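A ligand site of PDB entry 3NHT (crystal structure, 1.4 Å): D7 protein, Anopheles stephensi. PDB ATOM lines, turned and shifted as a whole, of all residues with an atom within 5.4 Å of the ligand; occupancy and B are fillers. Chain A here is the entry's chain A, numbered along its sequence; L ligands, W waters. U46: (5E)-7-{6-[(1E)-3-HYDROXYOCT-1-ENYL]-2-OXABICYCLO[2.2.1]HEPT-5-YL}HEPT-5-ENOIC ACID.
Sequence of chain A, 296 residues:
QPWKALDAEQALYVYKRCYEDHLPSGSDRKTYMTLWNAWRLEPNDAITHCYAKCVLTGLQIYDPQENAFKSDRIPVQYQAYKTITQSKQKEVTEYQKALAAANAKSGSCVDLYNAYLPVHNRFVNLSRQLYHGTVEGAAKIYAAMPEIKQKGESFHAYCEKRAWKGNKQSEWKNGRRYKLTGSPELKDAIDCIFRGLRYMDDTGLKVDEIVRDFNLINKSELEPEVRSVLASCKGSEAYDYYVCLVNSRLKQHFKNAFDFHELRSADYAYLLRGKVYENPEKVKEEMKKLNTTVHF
The side-chain amino group of Lys 151 is in salt-bridge range of an oxygen (OAY) of the ligand (2.7 Å).
The side-chain hydroxyl of Tyr 51 lies within hydrogen-bond range of an oxygen (OAU) of the ligand (2.7 Å).
O of Trp 36 sits at hydrogen-bond distance from OAU of the ligand (2.7 Å).
The backbone carbonyl oxygen of Arg 128 lies within hydrogen-bond range of the backbone NH of Gly 133, at 2.8 Å.
The backbone carbonyl oxygen (O) of Trp 36 lies close to the side-chain hydroxyl (OH) of Tyr 19, 3.5 Å away.
O of Trp 39 is in hydrogen-bond range of NE2 of His 120, 2.8 Å away.
The side-chain hydroxyl (OH) of Tyr 19 is in hydrogen-bond range of the side-chain amide oxygen (OD1) of Asn 37 (2.7 Å).
Residues that only touch the ligand: Leu 12 (3.7 Å), Tyr 15 (3.3 Å), Tyr 19 (3.6 Å), Asn 37 (3.9 Å), Trp 39 (3.3 Å), Leu 41 (3.8 Å), Ala 52 (3.9 Å), Val 55 (3.7 Å), His 120 (3.97 Å), His 132 (3.4 Å), Gly 133 (3.1 Å), Thr 134 (3.5 Å), Val 135 (3.7 Å) and Ala 138 (3.8 Å).
Water W1 bridges the side-chain hydroxyl (OH) of Tyr 142 and an oxygen (OAX) of the ligand.
Water W3 lies within hydrogen-bond range of an oxygen (OAX) of the ligand, the backbone carbonyl oxygen (O) of Val 135 and the backbone NH (N) of Ala 139.
Water W5 lies within hydrogen-bond range of OAS of the ligand (2.9 Å), O of Leu 12 (3.1 Å) and N of Lys 16 (3.4 Å).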
ATOM      1  N   LEU A  12     -11.081 -14.597 -15.463  1.00  0.00           N
ATOM      2  CA  LEU A  12     -11.440 -13.253 -15.013  1.00  0.00           C
ATOM      3  C   LEU A  12     -12.758 -12.803 -15.634  1.00  0.00           C
ATOM      4  O   LEU A  12     -13.581 -12.146 -14.971  1.00  0.00           O
ATOM      5  CB  LEU A  12     -10.318 -12.251 -15.340  1.00  0.00           C
ATOM      6  CG  LEU A  12     -10.401 -10.897 -14.619  1.00  0.00           C
ATOM      7  CD1 LEU A  12     -10.216 -11.062 -13.099  1.00  0.00           C
ATOM      8  CD2 LEU A  12      -9.368  -9.939 -15.168  1.00  0.00           C
ATOM      9  N   TYR A  15     -15.624 -14.441 -13.681  1.00  0.00           N
ATOM     10  CA  TYR A  15     -15.868 -13.814 -12.387  1.00  0.00           C
ATOM     11  C   TYR A  15     -16.571 -12.479 -12.544  1.00  0.00           C
ATOM     12  O   TYR A  15     -17.540 -12.199 -11.844  1.00  0.00           O
ATOM     13  CB  TYR A  15     -14.575 -13.645 -11.562  1.00  0.00           C
ATOM     14  CG  TYR A  15     -13.780 -14.924 -11.336  1.00  0.00           C
ATOM     15  CD1 TYR A  15     -14.397 -16.078 -10.839  1.00  0.00           C
ATOM     16  CD2 TYR A  15     -12.407 -14.961 -11.582  1.00  0.00           C
ATOM     17  CE1 TYR A  15     -13.675 -17.251 -10.637  1.00  0.00           C
ATOM     18  CE2 TYR A  15     -11.676 -16.136 -11.381  1.00  0.00           C
ATOM     19  CZ  TYR A  15     -12.320 -17.266 -10.906  1.00  0.00           C
ATOM     20  OH  TYR A  15     -11.617 -18.432 -10.702  1.00  0.00           O
ATOM     21  N   LYS A  16     -16.095 -11.652 -13.480  1.00  0.00           N
ATOM     22  CA  LYS A  16     -16.648 -10.299 -13.607  1.00  0.00           C
ATOM     23  C   LYS A  16     -18.067 -10.323 -14.164  1.00  0.00           C
ATOM     24  O   LYS A  16     -18.915  -9.566 -13.698  1.00  0.00           O
ATOM     25  CB  LYS A  16     -15.724  -9.349 -14.384  1.00  0.00           C
ATOM     26  CG  LYS A  16     -15.595  -9.611 -15.883  1.00  0.00           C
ATOM     27  CD  LYS A  16     -16.409  -8.607 -16.709  1.00  0.00           C
ATOM     28  CE  LYS A  16     -16.141  -8.809 -18.202  1.00  0.00           C
ATOM     29  NZ  LYS A  16     -16.899  -7.852 -19.050  1.00  0.00           N
ATOM     30  N   TYR A  19     -20.285 -11.341 -11.308  1.00  0.00           N
ATOM     31  CA  TYR A  19     -20.530 -10.171 -10.446  1.00  0.00           C
ATOM     32  C   TYR A  19     -21.571  -9.259 -11.071  1.00  0.00           C
ATOM     33  O   TYR A  19     -22.517  -8.834 -10.405  1.00  0.00           O
ATOM     34  CB  TYR A  19     -19.233  -9.385 -10.207  1.00  0.00           C
ATOM     35  CG  TYR A  19     -18.396  -9.797  -8.995  1.00  0.00           C
ATOM     36  CD1 TYR A  19     -17.805  -8.837  -8.194  1.00  0.00           C
ATOM     37  CD2 TYR A  19     -18.176 -11.138  -8.684  1.00  0.00           C
ATOM     38  CE1 TYR A  19     -17.026  -9.188  -7.090  1.00  0.00           C
ATOM     39  CE2 TYR A  19     -17.401 -11.497  -7.584  1.00  0.00           C
ATOM     40  CZ  TYR A  19     -16.836 -10.513  -6.806  1.00  0.00           C
ATOM     41  OH  TYR A  19     -16.067 -10.884  -5.724  1.00  0.00           O
ATOM     42  N   TRP A  36     -17.619 -12.146  -1.459  1.00  0.00           N
ATOM     43  CA  TRP A  36     -17.226 -12.870  -2.672  1.00  0.00           C
ATOM     44  C   TRP A  36     -15.779 -12.563  -3.079  1.00  0.00           C
ATOM     45  O   TRP A  36     -15.101 -13.453  -3.593  1.00  0.00           O
ATOM     46  CB  TRP A  36     -18.197 -12.592  -3.828  1.00  0.00           C
ATOM     47  CG  TRP A  36     -19.645 -12.914  -3.544  1.00  0.00           C
ATOM     48  CD1 TRP A  36     -20.159 -13.595  -2.471  1.00  0.00           C
ATOM     49  CD2 TRP A  36     -20.757 -12.559  -4.366  1.00  0.00           C
ATOM     50  NE1 TRP A  36     -21.529 -13.687  -2.582  1.00  0.00           N
ATOM     51  CE2 TRP A  36     -21.919 -13.058  -3.730  1.00  0.00           C
ATOM     52  CE3 TRP A  36     -20.889 -11.867  -5.580  1.00  0.00           C
ATOM     53  CZ2 TRP A  36     -23.201 -12.874  -4.279  1.00  0.00           C
ATOM     54  CZ3 TRP A  36     -22.157 -11.708  -6.119  1.00  0.00           C
ATOM     55  CH2 TRP A  36     -23.290 -12.193  -5.462  1.00  0.00           C
ATOM     56  N   ASN A  37     -15.303 -11.343  -2.838  1.00  0.00           N
ATOM     57  CA  ASN A  37     -13.899 -11.011  -3.085  1.00  0.00           C
ATOM     58  C   ASN A  37     -12.957 -11.912  -2.276  1.00  0.00           C
ATOM     59  O   ASN A  37     -11.854 -12.247  -2.723  1.00  0.00           O
ATOM     60  CB  ASN A  37     -13.602  -9.557  -2.712  1.00  0.00           C
ATOM     61  CG  ASN A  37     -14.077  -8.546  -3.734  1.00  0.00           C
ATOM     62  OD1 ASN A  37     -14.549  -8.891  -4.818  1.00  0.00           O
ATOM     63  ND2 ASN A  37     -13.949  -7.265  -3.385  1.00  0.00           N
ATOM     64  N   TRP A  39     -13.621 -14.962  -1.547  1.00  0.00           N
ATOM     65  CA  TRP A  39     -13.977 -16.359  -1.869  1.00  0.00           C
ATOM     66  C   TRP A  39     -14.766 -17.030  -0.737  1.00  0.00           C
ATOM     67  O   TRP A  39     -14.598 -18.211  -0.431  1.00  0.00           O
ATOM     68  CB  TRP A  39     -12.721 -17.160  -2.280  1.00  0.00           C
ATOM     69  CG  TRP A  39     -12.270 -16.808  -3.675  1.00  0.00           C
ATOM     70  CD1 TRP A  39     -11.794 -15.603  -4.093  1.00  0.00           C
ATOM     71  CD2 TRP A  39     -12.256 -17.671  -4.814  1.00  0.00           C
ATOM     72  NE1 TRP A  39     -11.475 -15.656  -5.433  1.00  0.00           N
ATOM     73  CE2 TRP A  39     -11.761 -16.913  -5.902  1.00  0.00           C
ATOM     74  CE3 TRP A  39     -12.621 -19.011  -5.036  1.00  0.00           C
ATOM     75  CZ2 TRP A  39     -11.619 -17.437  -7.190  1.00  0.00           C
ATOM     76  CZ3 TRP A  39     -12.470 -19.539  -6.326  1.00  0.00           C
ATOM     77  CH2 TRP A  39     -11.984 -18.759  -7.379  1.00  0.00           C
ATOM     78  N   LEU A  41     -18.526 -18.051   0.162  1.00  0.00           N
ATOM     79  CA  LEU A  41     -19.845 -18.260  -0.446  1.00  0.00           C
ATOM     80  C   LEU A  41     -20.929 -17.954   0.593  1.00  0.00           C
ATOM     81  O   LEU A  41     -21.640 -18.842   1.061  1.00  0.00           O
ATOM     82  CB  LEU A  41     -19.978 -19.680  -1.020  1.00  0.00           C
ATOM     83  CG  LEU A  41     -19.110 -19.981  -2.250  1.00  0.00           C
ATOM     84  CD1 LEU A  41     -19.301 -21.427  -2.716  1.00  0.00           C
ATOM     85  CD2 LEU A  41     -19.421 -19.006  -3.375  1.00  0.00           C
ATOM     86  N   TYR A  51     -25.161 -16.792  -7.734  1.00  0.00           N
ATOM     87  CA  TYR A  51     -23.790 -16.385  -8.021  1.00  0.00           C
ATOM     88  C   TYR A  51     -22.886 -17.617  -8.129  1.00  0.00           C
ATOM     89  O   TYR A  51     -22.128 -17.750  -9.100  1.00  0.00           O
ATOM     90  CB  TYR A  51     -23.260 -15.392  -6.976  1.00  0.00           C
ATOM     91  CG  TYR A  51     -21.775 -15.167  -7.140  1.00  0.00           C
ATOM     92  CD1 TYR A  51     -21.274 -14.504  -8.258  1.00  0.00           C
ATOM     93  CD2 TYR A  51     -20.865 -15.635  -6.185  1.00  0.00           C
ATOM     94  CE1 TYR A  51     -19.908 -14.313  -8.424  1.00  0.00           C
ATOM     95  CE2 TYR A  51     -19.497 -15.445  -6.329  1.00  0.00           C
ATOM     96  CZ  TYR A  51     -19.044 -14.789  -7.464  1.00  0.00           C
ATOM     97  OH  TYR A  51     -17.699 -14.613  -7.674  1.00  0.00           O
ATOM     98  N   ALA A  52     -22.987 -18.515  -7.155  1.00  0.00           N
ATOM     99  CA  ALA A  52     -22.198 -19.747  -7.176  1.00  0.00           C
ATOM    100  C   ALA A  52     -22.488 -20.577  -8.427  1.00  0.00           C
ATOM    101  O   ALA A  52     -21.554 -21.036  -9.090  1.00  0.00           O
ATOM    102  CB  ALA A  52     -22.448 -20.573  -5.919  1.00  0.00           C
ATOM    103  N   VAL A  55     -20.711 -19.017 -11.430  1.00  0.00           N
ATOM    104  CA  VAL A  55     -19.278 -19.221 -11.514  1.00  0.00           C
ATOM    105  C   VAL A  55     -18.965 -20.676 -11.866  1.00  0.00           C
ATOM    106  O   VAL A  55     -18.102 -20.924 -12.714  1.00  0.00           O
ATOM    107  CB  VAL A  55     -18.539 -18.762 -10.250  1.00  0.00           C
ATOM    108  CG1 VAL A  55     -17.044 -19.059 -10.347  1.00  0.00           C
ATOM    109  CG2 VAL A  55     -18.772 -17.275 -10.012  1.00  0.00           C
ATOM    110  N   LEU A  56     -19.674 -21.621 -11.236  1.00  0.00           N
ATOM    111  CA  LEU A  56     -19.489 -23.032 -11.549  1.00  0.00           C
ATOM    112  C   LEU A  56     -19.749 -23.311 -13.032  1.00  0.00           C
ATOM    113  O   LEU A  56     -19.027 -24.090 -13.664  1.00  0.00           O
ATOM    114  CB  LEU A  56     -20.360 -23.933 -10.662  1.00  0.00           C
ATOM    115  CG  LEU A  56     -19.993 -23.962  -9.172  1.00  0.00           C
ATOM    116  CD1 LEU A  56     -21.130 -24.504  -8.330  1.00  0.00           C
ATOM    117  CD2 LEU A  56     -18.728 -24.775  -8.949  1.00  0.00           C
ATOM    118  N   TYR A 116     -21.861 -27.952  -3.777  1.00  0.00           N
ATOM    119  CA  TYR A 116     -20.496 -27.467  -3.919  1.00  0.00           C
ATOM    120  C   TYR A 116     -19.906 -26.885  -2.651  1.00  0.00           C
ATOM    121  O   TYR A 116     -18.696 -26.910  -2.476  1.00  0.00           O
ATOM    122  CB  TYR A 116     -20.396 -26.464  -5.075  1.00  0.00           C
ATOM    123  CG  TYR A 116     -18.965 -26.134  -5.424  1.00  0.00           C
ATOM    124  CD1 TYR A 116     -18.139 -27.088  -6.022  1.00  0.00           C
ATOM    125  CD2 TYR A 116     -18.428 -24.880  -5.138  1.00  0.00           C
ATOM    126  CE1 TYR A 116     -16.809 -26.795  -6.317  1.00  0.00           C
ATOM    127  CE2 TYR A 116     -17.107 -24.579  -5.440  1.00  0.00           C
ATOM    128  CZ  TYR A 116     -16.304 -25.544  -6.023  1.00  0.00           C
ATOM    129  OH  TYR A 116     -14.988 -25.261  -6.313  1.00  0.00           O
ATOM    130  N   HIS A 120     -15.976 -26.520  -1.914  1.00  0.00           N
ATOM    131  CA  HIS A 120     -15.392 -25.196  -1.849  1.00  0.00           C
ATOM    132  C   HIS A 120     -14.656 -24.955  -0.523  1.00  0.00           C
ATOM    133  O   HIS A 120     -13.515 -24.496  -0.518  1.00  0.00           O
ATOM    134  CB  HIS A 120     -16.493 -24.153  -1.994  1.00  0.00           C
ATOM    135  CG  HIS A 120     -16.019 -22.755  -1.826  1.00  0.00           C
ATOM    136  ND1 HIS A 120     -15.397 -22.033  -2.836  1.00  0.00           N
ATOM    137  CD2 HIS A 120     -16.074 -21.923  -0.752  1.00  0.00           C
ATOM    138  CE1 HIS A 120     -15.092 -20.835  -2.387  1.00  0.00           C
ATOM    139  NE2 HIS A 120     -15.502 -20.733  -1.128  1.00  0.00           N
ATOM    140  N   ARG A 128      -8.484 -21.643  -6.274  1.00  0.00           N
ATOM    141  CA  ARG A 128      -7.969 -20.338  -6.659  1.00  0.00           C
ATOM    142  C   ARG A 128      -6.659 -20.432  -7.443  1.00  0.00           C
ATOM    143  O   ARG A 128      -6.384 -19.575  -8.282  1.00  0.00           O
ATOM    144  CB  ARG A 128      -7.805 -19.426  -5.437  1.00  0.00           C
ATOM    145  CG  ARG A 128      -9.127 -19.155  -4.716  1.00  0.00           C
ATOM    146  CD  ARG A 128      -8.966 -18.198  -3.550  1.00  0.00           C
ATOM    147  NE  ARG A 128      -8.663 -16.855  -4.016  1.00  0.00           N
ATOM    148  CZ  ARG A 128      -8.627 -15.761  -3.250  1.00  0.00           C
ATOM    149  NH1 ARG A 128      -8.881 -15.842  -1.958  1.00  0.00           N
ATOM    150  NH2 ARG A 128      -8.352 -14.590  -3.801  1.00  0.00           N
ATOM    151  N   HIS A 132      -7.149 -19.513 -11.569  1.00  0.00           N
ATOM    152  CA  HIS A 132      -6.609 -18.161 -11.732  1.00  0.00           C
ATOM    153  C   HIS A 132      -7.399 -17.155 -10.932  1.00  0.00           C
ATOM    154  O   HIS A 132      -7.789 -16.080 -11.422  1.00  0.00           O
ATOM    155  CB  HIS A 132      -6.539 -17.820 -13.233  1.00  0.00           C
ATOM    156  CG  HIS A 132      -6.042 -18.951 -14.071  1.00  0.00           C
ATOM    157  ND1 HIS A 132      -4.852 -19.597 -13.806  1.00  0.00           N
ATOM    158  CD2 HIS A 132      -6.589 -19.577 -15.144  1.00  0.00           C
ATOM    159  CE1 HIS A 132      -4.679 -20.565 -14.686  1.00  0.00           C
ATOM    160  NE2 HIS A 132      -5.701 -20.564 -15.516  1.00  0.00           N
ATOM    161  N   GLY A 133      -7.625 -17.510  -9.676  1.00  0.00           N
ATOM    162  CA  GLY A 133      -8.406 -16.719  -8.742  1.00  0.00           C
ATOM    163  C   GLY A 133      -7.601 -15.988  -7.679  1.00  0.00           C
ATOM    164  O   GLY A 133      -8.120 -15.700  -6.598  1.00  0.00           O
ATOM    165  N   THR A 134      -6.335 -15.697  -7.966  1.00  0.00           N
ATOM    166  CA  THR A 134      -5.520 -14.816  -7.129  1.00  0.00           C
ATOM    167  C   THR A 134      -4.819 -13.841  -8.040  1.00  0.00           C
ATOM    168  O   THR A 134      -4.471 -14.171  -9.177  1.00  0.00           O
ATOM    169  CB  THR A 134      -4.441 -15.576  -6.303  1.00  0.00           C
ATOM    170  OG1 THR A 134      -3.423 -16.106  -7.183  1.00  0.00           O
ATOM    171  CG2 THR A 134      -5.053 -16.695  -5.466  1.00  0.00           C
ATOM    172  N   VAL A 135      -4.566 -12.636  -7.522  1.00  0.00           N
ATOM    173  CA  VAL A 135      -3.853 -11.616  -8.305  1.00  0.00           C
ATOM    174  C   VAL A 135      -2.443 -12.112  -8.677  1.00  0.00           C
ATOM    175  O   VAL A 135      -2.039 -12.021  -9.841  1.00  0.00           O
ATOM    176  CB  VAL A 135      -3.832 -10.247  -7.559  1.00  0.00           C
ATOM    177  CG1 VAL A 135      -2.982  -9.214  -8.316  1.00  0.00           C
ATOM    178  CG2 VAL A 135      -5.255  -9.728  -7.346  1.00  0.00           C
ATOM    179  N   ALA A 138      -2.576 -15.197 -11.188  1.00  0.00           N
ATOM    180  CA  ALA A 138      -2.955 -14.761 -12.545  1.00  0.00           C
ATOM    181  C   ALA A 138      -1.801 -13.998 -13.207  1.00  0.00           C
ATOM    182  O   ALA A 138      -1.563 -14.184 -14.407  1.00  0.00           O
ATOM    183  CB  ALA A 138      -4.234 -13.930 -12.531  1.00  0.00           C
ATOM    184  N   ALA A 139      -1.093 -13.182 -12.434  1.00  0.00           N
ATOM    185  CA  ALA A 139       0.021 -12.417 -13.006  1.00  0.00           C
ATOM    186  C   ALA A 139       1.064 -13.367 -13.579  1.00  0.00           C
ATOM    187  O   ALA A 139       1.658 -13.080 -14.624  1.00  0.00           O
ATOM    188  CB  ALA A 139       0.637 -11.477 -11.974  1.00  0.00           C
ATOM    189  N   TYR A 142      -0.182 -14.539 -17.036  1.00  0.00           N
ATOM    190  CA  TYR A 142       0.014 -13.521 -18.076  1.00  0.00           C
ATOM    191  C   TYR A 142       1.477 -13.413 -18.489  1.00  0.00           C
ATOM    192  O   TYR A 142       1.782 -13.291 -19.675  1.00  0.00           O
ATOM    193  CB  TYR A 142      -0.486 -12.150 -17.631  1.00  0.00           C
ATOM    194  CG  TYR A 142      -1.979 -12.076 -17.427  1.00  0.00           C
ATOM    195  CD1 TYR A 142      -2.861 -12.253 -18.497  1.00  0.00           C
ATOM    196  CD2 TYR A 142      -2.511 -11.774 -16.167  1.00  0.00           C
ATOM    197  CE1 TYR A 142      -4.230 -12.183 -18.313  1.00  0.00           C
ATOM    198  CE2 TYR A 142      -3.883 -11.685 -15.972  1.00  0.00           C
ATOM    199  CZ  TYR A 142      -4.744 -11.893 -17.047  1.00  0.00           C
ATOM    200  OH  TYR A 142      -6.113 -11.818 -16.871  1.00  0.00           O
ATOM    201  N   LYS A 151      -4.850  -7.431 -18.533  1.00  0.00           N
ATOM    202  CA  LYS A 151      -5.638  -6.397 -17.866  1.00  0.00           C
ATOM    203  C   LYS A 151      -5.112  -5.046 -18.361  1.00  0.00           C
ATOM    204  O   LYS A 151      -3.911  -4.881 -18.574  1.00  0.00           O
ATOM    205  CB  LYS A 151      -5.510  -6.452 -16.346  1.00  0.00           C
ATOM    206  CG  LYS A 151      -6.102  -7.696 -15.669  1.00  0.00           C
ATOM    207  CD  LYS A 151      -6.120  -7.496 -14.141  1.00  0.00           C
ATOM    208  CE  LYS A 151      -4.713  -7.450 -13.573  1.00  0.00           C
ATOM    209  NZ  LYS A 151      -4.680  -6.928 -12.174  1.00  0.00           N
ATOM    210  N   LEU A 272     -18.164  -3.095 -11.697  1.00  0.00           N
ATOM    211  CA  LEU A 272     -18.349  -3.927 -10.497  1.00  0.00           C
ATOM    212  C   LEU A 272     -18.720  -3.162  -9.224  1.00  0.00           C
ATOM    213  O   LEU A 272     -19.448  -3.695  -8.379  1.00  0.00           O
ATOM    214  CB  LEU A 272     -17.150  -4.846 -10.256  1.00  0.00           C
ATOM    215  CG  LEU A 272     -16.781  -5.824 -11.394  1.00  0.00           C
ATOM    216  CD1 LEU A 272     -15.840  -6.915 -10.896  1.00  0.00           C
ATOM    217  CD2 LEU A 272     -17.998  -6.445 -12.087  1.00  0.00           C
HETATM  218  OAX U46 L   1      -5.658 -10.380 -12.245  1.00  0.00           O
HETATM  219  CAW U46 L   1      -6.489  -9.853 -11.242  1.00  0.00           C
HETATM  220  OAY U46 L   1      -6.414  -8.521 -10.857  1.00  0.00           O
HETATM  221  CAR U46 L   1      -7.542 -10.720 -10.518  1.00  0.00           C
HETATM  222  CAQ U46 L   1      -7.187 -12.199 -10.665  1.00  0.00           C
HETATM  223  CAP U46 L   1      -8.296 -13.020  -9.998  1.00  0.00           C
HETATM  224  CAO U46 L   1      -8.180 -12.801  -8.476  1.00  0.00           C
HETATM  225  CAN U46 L   1      -9.377 -13.050  -7.715  1.00  0.00           C
HETATM  226  CAF U46 L   1     -10.728 -13.495  -8.272  1.00  0.00           C
HETATM  227  CAD U46 L   1     -11.803 -12.666  -7.550  1.00  0.00           C
HETATM  228  CAC U46 L   1     -11.669 -11.162  -7.787  1.00  0.00           C
HETATM  229  CAB U46 L   1     -13.024 -10.573  -8.024  1.00  0.00           C
HETATM  230  CAT U46 L   1     -11.859 -10.812  -9.261  1.00  0.00           C
HETATM  231  OAS U46 L   1     -13.178 -11.206  -9.868  1.00  0.00           O
HETATM  232  CAA U46 L   1     -13.922 -11.669  -8.618  1.00  0.00           C
HETATM  233  CAE U46 L   1     -13.225 -12.922  -8.085  1.00  0.00           C
HETATM  234  CAG U46 L   1     -14.089 -13.692  -7.091  1.00  0.00           C
HETATM  235  CAH U46 L   1     -14.204 -15.117  -7.221  1.00  0.00           C
HETATM  236  CAI U46 L   1     -15.030 -15.853  -6.184  1.00  0.00           C
HETATM  237  OAU U46 L   1     -16.135 -15.070  -5.489  1.00  0.00           O
HETATM  238  CAJ U46 L   1     -15.460 -17.246  -6.587  1.00  0.00           C
HETATM  239  CAK U46 L   1     -16.083 -18.084  -5.459  1.00  0.00           C
HETATM  240  CAL U46 L   1     -16.591 -19.480  -5.799  1.00  0.00           C
HETATM  241  CAM U46 L   1     -17.807 -19.607  -6.710  1.00  0.00           C
HETATM  242  CAV U46 L   1     -18.233 -21.035  -7.075  1.00  0.00           C
HETATM  243  O   HOH W   1      -6.642 -11.926 -14.260  1.00  0.00           O
HETATM  244  O   HOH W   2      -7.976  -7.481  -9.095  1.00  0.00           O
HETATM  245  O   HOH W   3      -2.907 -10.480 -12.008  1.00  0.00           O
HETATM  246  O   HOH W   4     -10.448 -11.012  -4.736  1.00  0.00           O
HETATM  247  O   HOH W   5     -13.196 -10.236 -12.569  1.00  0.00           O
